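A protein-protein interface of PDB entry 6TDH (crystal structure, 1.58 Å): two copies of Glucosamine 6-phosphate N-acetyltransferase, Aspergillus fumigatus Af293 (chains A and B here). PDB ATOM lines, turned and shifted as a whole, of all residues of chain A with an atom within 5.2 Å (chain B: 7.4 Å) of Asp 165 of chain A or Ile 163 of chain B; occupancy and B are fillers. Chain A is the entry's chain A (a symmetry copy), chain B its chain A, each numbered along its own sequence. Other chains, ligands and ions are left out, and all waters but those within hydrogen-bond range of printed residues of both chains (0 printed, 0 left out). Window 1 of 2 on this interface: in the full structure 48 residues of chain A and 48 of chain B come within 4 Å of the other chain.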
ATOM      1  N   ILE A 128      -5.008  24.162   1.086  1.00  0.00           N
ATOM      2  CA  ILE A 128      -6.451  24.422   0.870  1.00  0.00           C
ATOM      3  C   ILE A 128      -6.907  25.544   1.797  1.00  0.00           C
ATOM      4  O   ILE A 128      -6.590  25.517   3.011  1.00  0.00           O
ATOM      5  CB  ILE A 128      -7.280  23.144   0.929  1.00  0.00           C
ATOM      6  CG1 ILE A 128      -6.996  22.324  -0.329  1.00  0.00           C
ATOM      7  CG2 ILE A 128      -8.766  23.456   1.078  1.00  0.00           C
ATOM      8  CD1 ILE A 128      -7.618  20.991  -0.334  1.00  0.00           C
ATOM      9  N   ILE A 163      -2.373  20.208   2.359  1.00  0.00           N
ATOM     10  CA  ILE A 163      -2.655  20.393   3.806  1.00  0.00           C
ATOM     11  C   ILE A 163      -3.680  21.514   3.962  1.00  0.00           C
ATOM     12  O   ILE A 163      -3.773  22.369   3.073  1.00  0.00           O
ATOM     13  CB  ILE A 163      -1.334  20.627   4.603  1.00  0.00           C
ATOM     14  CG1 ILE A 163      -0.535  21.840   4.140  1.00  0.00           C
ATOM     15  CG2 ILE A 163      -0.481  19.353   4.534  1.00  0.00           C
ATOM     16  CD1 ILE A 163       0.571  22.268   5.137  1.00  0.00           C
ATOM     17  N   LEU A 164      -4.300  21.572   5.124  1.00  0.00           N
ATOM     18  CA  LEU A 164      -5.183  22.693   5.508  1.00  0.00           C
ATOM     19  C   LEU A 164      -5.214  22.719   7.039  1.00  0.00           C
ATOM     20  O   LEU A 164      -4.844  21.738   7.675  1.00  0.00           O
ATOM     21  CB  LEU A 164      -6.582  22.527   4.898  1.00  0.00           C
ATOM     22  CG  LEU A 164      -7.312  21.237   5.264  1.00  0.00           C
ATOM     23  CD1 LEU A 164      -8.074  21.346   6.588  1.00  0.00           C
ATOM     24  CD2 LEU A 164      -8.250  20.783   4.139  1.00  0.00           C
ATOM     25  N   ASP A 165      -5.643  23.834   7.574  1.00  0.00           N
ATOM     26  CA  ASP A 165      -5.879  24.013   9.013  1.00  0.00           C
ATOM     27  C   ASP A 165      -7.388  24.074   9.209  1.00  0.00           C
ATOM     28  O   ASP A 165      -8.093  24.755   8.406  1.00  0.00           O
ATOM     29  CB  ASP A 165      -5.202  25.278   9.503  1.00  0.00           C
ATOM     30  CG  ASP A 165      -3.689  25.199   9.415  1.00  0.00           C
ATOM     31  OD1 ASP A 165      -3.109  24.117   9.725  1.00  0.00           O
ATOM     32  OD2 ASP A 165      -3.114  26.209   9.002  1.00  0.00           O
ATOM     33  N   CYS A 166      -7.864  23.465  10.265  1.00  0.00           N
ATOM     34  CA  CYS A 166      -9.305  23.532  10.566  1.00  0.00           C
ATOM     35  C   CYS A 166      -9.509  23.643  12.073  1.00  0.00           C
ATOM     36  O   CYS A 166      -8.560  23.418  12.828  1.00  0.00           O
ATOM     37  CB  CYS A 166      -9.999  22.334   9.938  1.00  0.00           C
ATOM     38  SG  CYS A 166      -9.635  20.767  10.738  1.00  0.00           S
ATOM     39  N   SER A 167     -10.714  24.041  12.466  1.00  0.00           N
ATOM     40  CA  SER A 167     -11.206  24.007  13.869  1.00  0.00           C
ATOM     41  C   SER A 167     -11.519  22.556  14.215  1.00  0.00           C
ATOM     42  O   SER A 167     -11.769  21.780  13.281  1.00  0.00           O
ATOM     43  CB  SER A 167     -12.440  24.872  14.028  1.00  0.00           C
ATOM     44  OG  SER A 167     -13.506  24.395  13.213  1.00  0.00           O
ATOM     45  N   TYR A 174     -13.532  17.437   7.033  1.00  0.00           N
ATOM     46  CA  TYR A 174     -12.274  17.077   6.329  1.00  0.00           C
ATOM     47  C   TYR A 174     -11.988  15.589   6.392  1.00  0.00           C
ATOM     48  O   TYR A 174     -11.418  15.038   5.445  1.00  0.00           O
ATOM     49  CB  TYR A 174     -11.115  17.948   6.830  1.00  0.00           C
ATOM     50  CG  TYR A 174     -11.399  19.402   6.581  1.00  0.00           C
ATOM     51  CD1 TYR A 174     -11.768  20.223   7.629  1.00  0.00           C
ATOM     52  CD2 TYR A 174     -11.409  19.922   5.292  1.00  0.00           C
ATOM     53  CE1 TYR A 174     -12.079  21.547   7.412  1.00  0.00           C
ATOM     54  CE2 TYR A 174     -11.736  21.252   5.066  1.00  0.00           C
ATOM     55  CZ  TYR A 174     -12.072  22.053   6.134  1.00  0.00           C
ATOM     56  OH  TYR A 174     -12.395  23.375   5.968  1.00  0.00           O
ATOM     57  N   GLU A 185      -2.054  23.418  14.303  1.00  0.00           N
ATOM     58  CA  GLU A 185      -1.934  24.807  13.819  1.00  0.00           C
ATOM     59  C   GLU A 185      -1.614  25.671  15.037  1.00  0.00           C
ATOM     60  O   GLU A 185      -2.369  25.622  16.032  1.00  0.00           O
ATOM     61  CB  GLU A 185      -3.220  25.272  13.149  1.00  0.00           C
ATOM     62  CG  GLU A 185      -3.177  26.682  12.640  1.00  0.00           C
ATOM     63  CD  GLU A 185      -4.495  27.353  12.282  1.00  0.00           C
ATOM     64  OE1 GLU A 185      -5.571  26.779  12.519  1.00  0.00           O
ATOM     65  OE2 GLU A 185      -4.428  28.478  11.801  1.00  0.00           O
ATOM     66  N   MET A 186      -0.518  26.408  14.966  1.00  0.00           N
ATOM     67  CA  MET A 186      -0.127  27.397  15.997  1.00  0.00           C
ATOM     68  C   MET A 186      -0.262  28.795  15.413  1.00  0.00           C
ATOM     69  O   MET A 186      -0.027  29.002  14.194  1.00  0.00           O
ATOM     70  CB  MET A 186       1.306  27.163  16.454  1.00  0.00           C
ATOM     71  CG  MET A 186       1.602  25.730  16.828  1.00  0.00           C
ATOM     72  SD  MET A 186       0.733  25.218  18.324  1.00  0.00           S
ATOM     73  CE  MET A 186       1.613  26.161  19.597  1.00  0.00           C
ATOM     74  N   ALA A 187      -0.622  29.759  16.248  1.00  0.00           N
ATOM     75  CA  ALA A 187      -0.880  31.115  15.764  1.00  0.00           C
ATOM     76  C   ALA A 187      -0.262  32.135  16.695  1.00  0.00           C
ATOM     77  O   ALA A 187      -0.151  31.892  17.906  1.00  0.00           O
ATOM     78  CB  ALA A 187      -2.355  31.351  15.618  1.00  0.00           C
ATOM     79  N   HIS A 188       0.098  33.263  16.115  1.00  0.00           N
ATOM     80  CA  HIS A 188       0.680  34.436  16.821  1.00  0.00           C
ATOM     81  C   HIS A 188      -0.046  35.658  16.308  1.00  0.00           C
ATOM     82  O   HIS A 188       0.006  35.900  15.104  1.00  0.00           O
ATOM     83  CB  HIS A 188       2.193  34.537  16.607  1.00  0.00           C
ATOM     84  CG  HIS A 188       2.836  35.664  17.357  1.00  0.00           C
ATOM     85  ND1 HIS A 188       3.392  35.506  18.594  1.00  0.00           N
ATOM     86  CD2 HIS A 188       3.062  36.950  17.009  1.00  0.00           C
ATOM     87  CE1 HIS A 188       3.909  36.655  19.003  1.00  0.00           C
ATOM     88  NE2 HIS A 188       3.706  37.563  18.053  1.00  0.00           N
ATOM     89  N   SER B 111      11.651  30.715   6.864  1.00  0.00           N
ATOM     90  CA  SER B 111      10.821  31.282   5.784  1.00  0.00           C
ATOM     91  C   SER B 111       9.523  31.823   6.367  1.00  0.00           C
ATOM     92  O   SER B 111       8.917  31.215   7.293  1.00  0.00           O
ATOM     93  CB  SER B 111      10.495  30.271   4.703  1.00  0.00           C
ATOM     94  OG  SER B 111      11.665  29.746   4.132  1.00  0.00           O
ATOM     95  N   LEU B 112       9.168  32.978   5.866  1.00  0.00           N
ATOM     96  CA  LEU B 112       7.828  33.542   6.015  1.00  0.00           C
ATOM     97  C   LEU B 112       7.227  33.625   4.617  1.00  0.00           C
ATOM     98  O   LEU B 112       7.840  34.254   3.723  1.00  0.00           O
ATOM     99  CB  LEU B 112       7.900  34.906   6.675  1.00  0.00           C
ATOM    100  CG  LEU B 112       6.528  35.589   6.752  1.00  0.00           C
ATOM    101  CD1 LEU B 112       5.735  34.978   7.887  1.00  0.00           C
ATOM    102  CD2 LEU B 112       6.658  37.080   6.945  1.00  0.00           C
ATOM    103  N   VAL B 113       6.069  33.024   4.418  1.00  0.00           N
ATOM    104  CA  VAL B 113       5.352  33.171   3.130  1.00  0.00           C
ATOM    105  C   VAL B 113       4.127  34.036   3.426  1.00  0.00           C
ATOM    106  O   VAL B 113       3.379  33.693   4.318  1.00  0.00           O
ATOM    107  CB  VAL B 113       4.987  31.824   2.500  1.00  0.00           C
ATOM    108  CG1 VAL B 113       4.259  32.022   1.184  1.00  0.00           C
ATOM    109  CG2 VAL B 113       6.220  30.969   2.319  1.00  0.00           C
ATOM    110  N   GLU B 115       0.691  35.446   2.469  1.00  0.00           N
ATOM    111  CA  GLU B 115      -0.488  35.086   1.660  1.00  0.00           C
ATOM    112  C   GLU B 115      -1.308  36.368   1.537  1.00  0.00           C
ATOM    113  O   GLU B 115      -1.812  36.845   2.544  1.00  0.00           O
ATOM    114  CB  GLU B 115      -1.235  33.957   2.372  1.00  0.00           C
ATOM    115  CG  GLU B 115      -2.393  33.376   1.574  1.00  0.00           C
ATOM    116  CD  GLU B 115      -3.338  32.501   2.392  1.00  0.00           C
ATOM    117  OE1 GLU B 115      -3.202  32.457   3.683  1.00  0.00           O
ATOM    118  OE2 GLU B 115      -4.261  31.905   1.751  1.00  0.00           O
ATOM    119  N   VAL B 125      -2.046  36.996   5.755  1.00  0.00           N
ATOM    120  CA  VAL B 125      -1.637  35.986   6.761  1.00  0.00           C
ATOM    121  C   VAL B 125      -0.195  35.599   6.461  1.00  0.00           C
ATOM    122  O   VAL B 125       0.104  35.252   5.324  1.00  0.00           O
ATOM    123  CB  VAL B 125      -2.560  34.751   6.688  1.00  0.00           C
ATOM    124  CG1 VAL B 125      -2.157  33.688   7.706  1.00  0.00           C
ATOM    125  CG2 VAL B 125      -4.010  35.193   6.917  1.00  0.00           C
ATOM    126  N   GLY B 126       0.655  35.648   7.484  1.00  0.00           N
ATOM    127  CA  GLY B 126       1.996  35.086   7.376  1.00  0.00           C
ATOM    128  C   GLY B 126       1.972  33.630   7.708  1.00  0.00           C
ATOM    129  O   GLY B 126       1.267  33.200   8.680  1.00  0.00           O
ATOM    130  N   HIS B 127       2.773  32.878   6.986  1.00  0.00           N
ATOM    131  CA  HIS B 127       2.957  31.432   7.213  1.00  0.00           C
ATOM    132  C   HIS B 127       4.430  31.174   7.462  1.00  0.00           C
ATOM    133  O   HIS B 127       5.215  31.384   6.526  1.00  0.00           O
ATOM    134  CB  HIS B 127       2.486  30.654   6.014  1.00  0.00           C
ATOM    135  CG  HIS B 127       1.058  30.876   5.704  1.00  0.00           C
ATOM    136  ND1 HIS B 127       0.084  30.068   6.215  1.00  0.00           N
ATOM    137  CD2 HIS B 127       0.436  31.864   5.028  1.00  0.00           C
ATOM    138  CE1 HIS B 127      -1.108  30.519   5.785  1.00  0.00           C
ATOM    139  NE2 HIS B 127      -0.910  31.596   5.056  1.00  0.00           N
ATOM    140  N   ILE B 128       4.739  30.694   8.657  1.00  0.00           N
ATOM    141  CA  ILE B 128       6.135  30.342   9.013  1.00  0.00           C
ATOM    142  C   ILE B 128       6.433  28.922   8.547  1.00  0.00           C
ATOM    143  O   ILE B 128       5.618  28.000   8.793  1.00  0.00           O
ATOM    144  CB  ILE B 128       6.443  30.631  10.478  1.00  0.00           C
ATOM    145  CG1 ILE B 128       6.524  32.145  10.667  1.00  0.00           C
ATOM    146  CG2 ILE B 128       7.727  29.936  10.919  1.00  0.00           C
ATOM    147  CD1 ILE B 128       6.669  32.572  12.068  1.00  0.00           C
ATOM    148  N   GLU B 129       7.570  28.747   7.865  1.00  0.00           N
ATOM    149  CA  GLU B 129       7.910  27.454   7.246  1.00  0.00           C
ATOM    150  C   GLU B 129       9.423  27.207   7.350  1.00  0.00           C
ATOM    151  O   GLU B 129      10.211  28.183   7.349  1.00  0.00           O
ATOM    152  CB  GLU B 129       7.556  27.412   5.757  1.00  0.00           C
ATOM    153  CG  GLU B 129       6.188  27.935   5.391  1.00  0.00           C
ATOM    154  CD  GLU B 129       5.073  26.955   5.664  1.00  0.00           C
ATOM    155  OE1 GLU B 129       5.399  25.769   5.852  1.00  0.00           O
ATOM    156  OE2 GLU B 129       3.886  27.377   5.712  1.00  0.00           O
ATOM    157  N   ASP B 151       8.330  36.886  12.644  1.00  0.00           N
ATOM    158  CA  ASP B 151       7.139  37.588  13.176  1.00  0.00           C
ATOM    159  C   ASP B 151       7.225  39.092  12.911  1.00  0.00           C
ATOM    160  O   ASP B 151       6.208  39.684  12.544  1.00  0.00           O
ATOM    161  CB  ASP B 151       6.943  37.281  14.651  1.00  0.00           C
ATOM    162  CG  ASP B 151       6.235  35.988  14.894  1.00  0.00           C
ATOM    163  OD1 ASP B 151       6.315  35.537  16.045  1.00  0.00           O
ATOM    164  OD2 ASP B 151       5.748  35.388  13.917  1.00  0.00           O
ATOM    165  N   LYS B 161      -1.837  38.193  11.446  1.00  0.00           N
ATOM    166  CA  LYS B 161      -1.420  37.035  12.255  1.00  0.00           C
ATOM    167  C   LYS B 161      -0.356  36.259  11.482  1.00  0.00           C
ATOM    168  O   LYS B 161      -0.311  36.413  10.243  1.00  0.00           O
ATOM    169  CB  LYS B 161      -2.606  36.140  12.602  1.00  0.00           C
ATOM    170  CG  LYS B 161      -3.214  35.375  11.448  1.00  0.00           C
ATOM    171  CD  LYS B 161      -4.381  34.482  11.875  1.00  0.00           C
ATOM    172  CE  LYS B 161      -4.816  33.604  10.725  1.00  0.00           C
ATOM    173  NZ  LYS B 161      -6.041  32.832  11.031  1.00  0.00           N
ATOM    174  N   THR B 162       0.448  35.512  12.237  1.00  0.00           N
ATOM    175  CA  THR B 162       1.307  34.483  11.639  1.00  0.00           C
ATOM    176  C   THR B 162       0.846  33.107  12.118  1.00  0.00           C
ATOM    177  O   THR B 162       0.517  32.943  13.309  1.00  0.00           O
ATOM    178  CB  THR B 162       2.776  34.763  11.905  1.00  0.00           C
ATOM    179  OG1 THR B 162       3.063  35.983  11.201  1.00  0.00           O
ATOM    180  CG2 THR B 162       3.655  33.655  11.401  1.00  0.00           C
ATOM    181  N   ILE B 163       0.798  32.164  11.208  1.00  0.00           N
ATOM    182  CA  ILE B 163       0.449  30.778  11.611  1.00  0.00           C
ATOM    183  C   ILE B 163       1.571  29.844  11.166  1.00  0.00           C
ATOM    184  O   ILE B 163       2.291  30.182  10.219  1.00  0.00           O
ATOM    185  CB  ILE B 163      -0.959  30.380  11.066  1.00  0.00           C
ATOM    186  CG1 ILE B 163      -1.082  30.454   9.548  1.00  0.00           C
ATOM    187  CG2 ILE B 163      -2.020  31.259  11.742  1.00  0.00           C
ATOM    188  CD1 ILE B 163      -2.339  29.738   8.995  1.00  0.00           C
ATOM    189  N   LEU B 164       1.599  28.658  11.741  1.00  0.00           N
ATOM    190  CA  LEU B 164       2.500  27.573  11.302  1.00  0.00           C
ATOM    191  C   LEU B 164       1.855  26.259  11.753  1.00  0.00           C
ATOM    192  O   LEU B 164       0.976  26.272  12.607  1.00  0.00           O
ATOM    193  CB  LEU B 164       3.911  27.759  11.880  1.00  0.00           C
ATOM    194  CG  LEU B 164       3.996  27.822  13.402  1.00  0.00           C
ATOM    195  CD1 LEU B 164       4.085  26.436  14.047  1.00  0.00           C
ATOM    196  CD2 LEU B 164       5.160  28.707  13.866  1.00  0.00           C
ATOM    197  N   ASP B 165       2.303  25.181  11.163  1.00  0.00           N
ATOM    198  CA  ASP B 165       1.916  23.816  11.547  1.00  0.00           C
ATOM    199  C   ASP B 165       3.126  23.189  12.225  1.00  0.00           C
ATOM    200  O   ASP B 165       4.277  23.356  11.722  1.00  0.00           O
ATOM    201  CB  ASP B 165       1.489  23.027  10.326  1.00  0.00           C
ATOM    202  CG  ASP B 165       0.221  23.573   9.694  1.00  0.00           C
ATOM    203  OD1 ASP B 165      -0.720  23.968  10.444  1.00  0.00           O
ATOM    204  OD2 ASP B 165       0.208  23.632   8.463  1.00  0.00           O
ATOM    205  N   CYS B 166       2.886  22.435  13.267  1.00  0.00           N
ATOM    206  CA  CYS B 166       3.995  21.734  13.940  1.00  0.00           C
ATOM    207  C   CYS B 166       3.530  20.353  14.389  1.00  0.00           C
ATOM    208  O   CYS B 166       2.325  20.091  14.385  1.00  0.00           O
ATOM    209  CB  CYS B 166       4.516  22.606  15.071  1.00  0.00           C
ATOM    210  SG  CYS B 166       3.401  22.743  16.473  1.00  0.00           S
ATOM    211  N   PHE B 179       3.644  31.437  20.468  1.00  0.00           N
ATOM    212  CA  PHE B 179       2.532  30.936  19.634  1.00  0.00           C
ATOM    213  C   PHE B 179       1.572  30.183  20.551  1.00  0.00           C
ATOM    214  O   PHE B 179       1.961  29.697  21.608  1.00  0.00           O
ATOM    215  CB  PHE B 179       3.024  30.052  18.490  1.00  0.00           C
ATOM    216  CG  PHE B 179       3.580  30.808  17.311  1.00  0.00           C
ATOM    217  CD1 PHE B 179       2.917  30.860  16.092  1.00  0.00           C
ATOM    218  CD2 PHE B 179       4.746  31.550  17.453  1.00  0.00           C
ATOM    219  CE1 PHE B 179       3.388  31.634  15.040  1.00  0.00           C
ATOM    220  CE2 PHE B 179       5.230  32.297  16.393  1.00  0.00           C
ATOM    221  CZ  PHE B 179       4.580  32.311  15.184  1.00  0.00           C
ATOM    222  N   ALA B 182      -4.162  26.825  17.760  1.00  0.00           N
ATOM    223  CA  ALA B 182      -5.263  27.548  17.101  1.00  0.00           C
ATOM    224  C   ALA B 182      -6.179  26.597  16.329  1.00  0.00           C
ATOM    225  O   ALA B 182      -7.254  27.026  15.920  1.00  0.00           O
ATOM    226  CB  ALA B 182      -4.693  28.586  16.178  1.00  0.00           C
ATOM    227  N   GLY B 183      -5.707  25.399  16.042  1.00  0.00           N
ATOM    228  CA  GLY B 183      -6.495  24.434  15.278  1.00  0.00           C
ATOM    229  C   GLY B 183      -5.664  23.216  15.005  1.00  0.00           C
ATOM    230  O   GLY B 183      -4.657  23.000  15.642  1.00  0.00           O
ATOM    231  N   LEU B 184      -6.110  22.420  14.035  1.00  0.00           N
ATOM    232  CA  LEU B 184      -5.491  21.149  13.642  1.00  0.00           C
ATOM    233  C   LEU B 184      -4.973  21.319  12.219  1.00  0.00           C
ATOM    234  O   LEU B 184      -5.635  22.010  11.418  1.00  0.00           O
ATOM    235  CB  LEU B 184      -6.559  20.054  13.639  1.00  0.00           C
ATOM    236  CG  LEU B 184      -7.285  19.878  14.966  1.00  0.00           C
ATOM    237  CD1 LEU B 184      -8.368  18.801  14.836  1.00  0.00           C
ATOM    238  CD2 LEU B 184      -6.294  19.533  16.057  1.00  0.00           C
ATOM    239  N   GLU B 185      -3.850  20.722  11.938  1.00  0.00           N
ATOM    240  CA  GLU B 185      -3.337  20.538  10.568  1.00  0.00           C
ATOM    241  C   GLU B 185      -3.899  19.212  10.061  1.00  0.00           C
ATOM    242  O   GLU B 185      -3.714  18.176  10.737  1.00  0.00           O
ATOM    243  CB  GLU B 185      -1.814  20.523  10.545  1.00  0.00           C
ATOM    244  CG  GLU B 185      -1.217  20.328   9.182  1.00  0.00           C
ATOM    245  CD  GLU B 185       0.255  19.947   9.093  1.00  0.00           C
ATOM    246  OE1 GLU B 185       0.896  19.696  10.126  1.00  0.00           O
ATOM    247  OE2 GLU B 185       0.734  19.865   7.969  1.00  0.00           O
ATOM    248  N   MET B 186      -4.585  19.255   8.931  1.00  0.00           N
ATOM    249  CA  MET B 186      -5.090  18.050   8.232  1.00  0.00           C
ATOM    250  C   MET B 186      -4.312  17.873   6.936  1.00  0.00           C
ATOM    251  O   MET B 186      -3.910  18.877   6.291  1.00  0.00           O
ATOM    252  CB  MET B 186      -6.576  18.184   7.930  1.00  0.00           C
ATOM    253  CG  MET B 186      -7.406  18.600   9.121  1.00  0.00           C
ATOM    254  SD  MET B 186      -7.480  17.317  10.387  1.00  0.00           S
ATOM    255  CE  MET B 186      -8.519  16.071   9.583  1.00  0.00           C
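The backbone NH of Ala 182 of chain B sits at hydrogen-bond distance from the backbone carbonyl oxygen of Glu 185 of chain A. O of Leu 164 of chain B lies within hydrogen-bond range of N of Met 186 of chain A, at 2.8 Å. The backbone carbonyl oxygen (O) of Thr 162 of chain B lies within hydrogen-bond range of the backbone NH (N) of His 188 of chain A (2.9 Å). The backbone NH (N) of Met 186 of chain B sits at hydrogen-bond distance from the backbone carbonyl oxygen (O) of Leu 164 of chain A (2.8 Å). The side-chain carboxylate (OD1) of Asp 165 of chain B lies close to the side-chain carboxylate (OD1) of Asp 165 of chain A. The backbone NH (N) of Cys 166 of chain A is in hydrogen-bond range of the backbone carbonyl oxygen (O) of Leu 184 of chain B (2.9 Å). The backbone carbonyl oxygen of Gly 183 of chain B is in hydrogen-bond range of the backbone NH of Glu 185 of chain A (3.0 Å).
The backbone carbonyl oxygen (O) of Ile 163 of chain A sits at hydrogen-bond distance from the backbone NH (N) of Ile 128 of chain A (2.9 Å). The backbone NH of Ile 163 of chain B lies within hydrogen-bond range of the backbone carbonyl oxygen of Gly 126 of chain B (2.8 Å). The backbone carbonyl oxygen of Ile 163 of chain B sits at hydrogen-bond distance from the backbone NH of Ile 128 of chain B. The backbone NH of Gly 126 of chain B sits at hydrogen-bond distance from the backbone carbonyl oxygen of Lys 161 of chain B (3.0 Å).
Ile 163 of chain A touches Glu 185 of chain B (CG2 to OE2, 3.7 Å). Met 186 of chain B touches Ile 163 of chain A (O to CA, 3.2 Å). O of Leu 164 of chain A touches O of Leu 184 of chain B, at 3.8 Å. Ile 163 of chain B touches Glu 185 of chain A. Glu 185 of chain A touches Leu 164 of chain B. CG of Met 186 of chain A touches SG of Cys 166 of chain B (3.5 Å). Ala 187 of chain A touches Thr 162 of chain B (CA to O, 3.4 Å). CB of Ala 187 of chain A touches CG2 of Ile 163 of chain B, at 3.9 Å. Phe 179 of chain B touches Ala 187 of chain A. Ala 187 of chain A touches Ala 182 of chain B.
Of chain B, only Ile 163 (3.6 Å), Asp 165 (2.5 Å), Leu 184 (3.1 Å) and Glu 185 (3.7 Å) come within 4 Å of Asp 165 of chain A. Of the printed residues of chain B, Glu 185 of chain A touches Ile 163, Leu 164, Asp 165, Ala 182 and Gly 183. Of the printed residues of chain B, His 188 of chain A touches Asp 151, Lys 161, Thr 162 and Phe 179. Ile 163 of chain B touches just these residues of chain A: Asp 165, Glu 185, Met 186 and Ala 187. Printed residues of chain A within 4 Å of Met 186 of chain B: Ile 163 (3.2 Å), Leu 164 (2.8 Å) and Cys 166 (3.5 Å). The nearest residue of chain B that does not touch Asp 165 of chain A is Met 186 of chain B (4.9 Å).
Hydrophobic or aromatic side chains of chain B within 4 Å of the printed part of chain A: Ile 163, Leu 164, Phe 179, Ala 182, Leu 184 and Met 186. Printed residues of chain A that touch a printed residue of chain B: Ile 163, Leu 164, Asp 165, Cys 166, Glu 185, Met 186, Ala 187 and His 188. Among the printed residues, no Asp or Glu carboxylate lies within 4 Å of a Lys or Arg side-chain nitrogen of the other chain.
Ile 163 of chain A touches Asp 165 of chain B, and with the chains exchanged Asp 165 of chain A touches Ile 163 of chain B. Ile 163 of chain A touches Met 186 of chain B, and with the chains exchanged Met 186 of chain A touches Ile 163 of chain B. Leu 164 of chain A touches Met 186 of chain B, and with the chains exchanged Met 186 of chain A touches Leu 164 of chain B. Cys 166 of chain A touches Met 186 of chain B, and with the chains exchanged Met 186 of chain A touches Cys 166 of chain B. 7 positions are printed for both chains.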
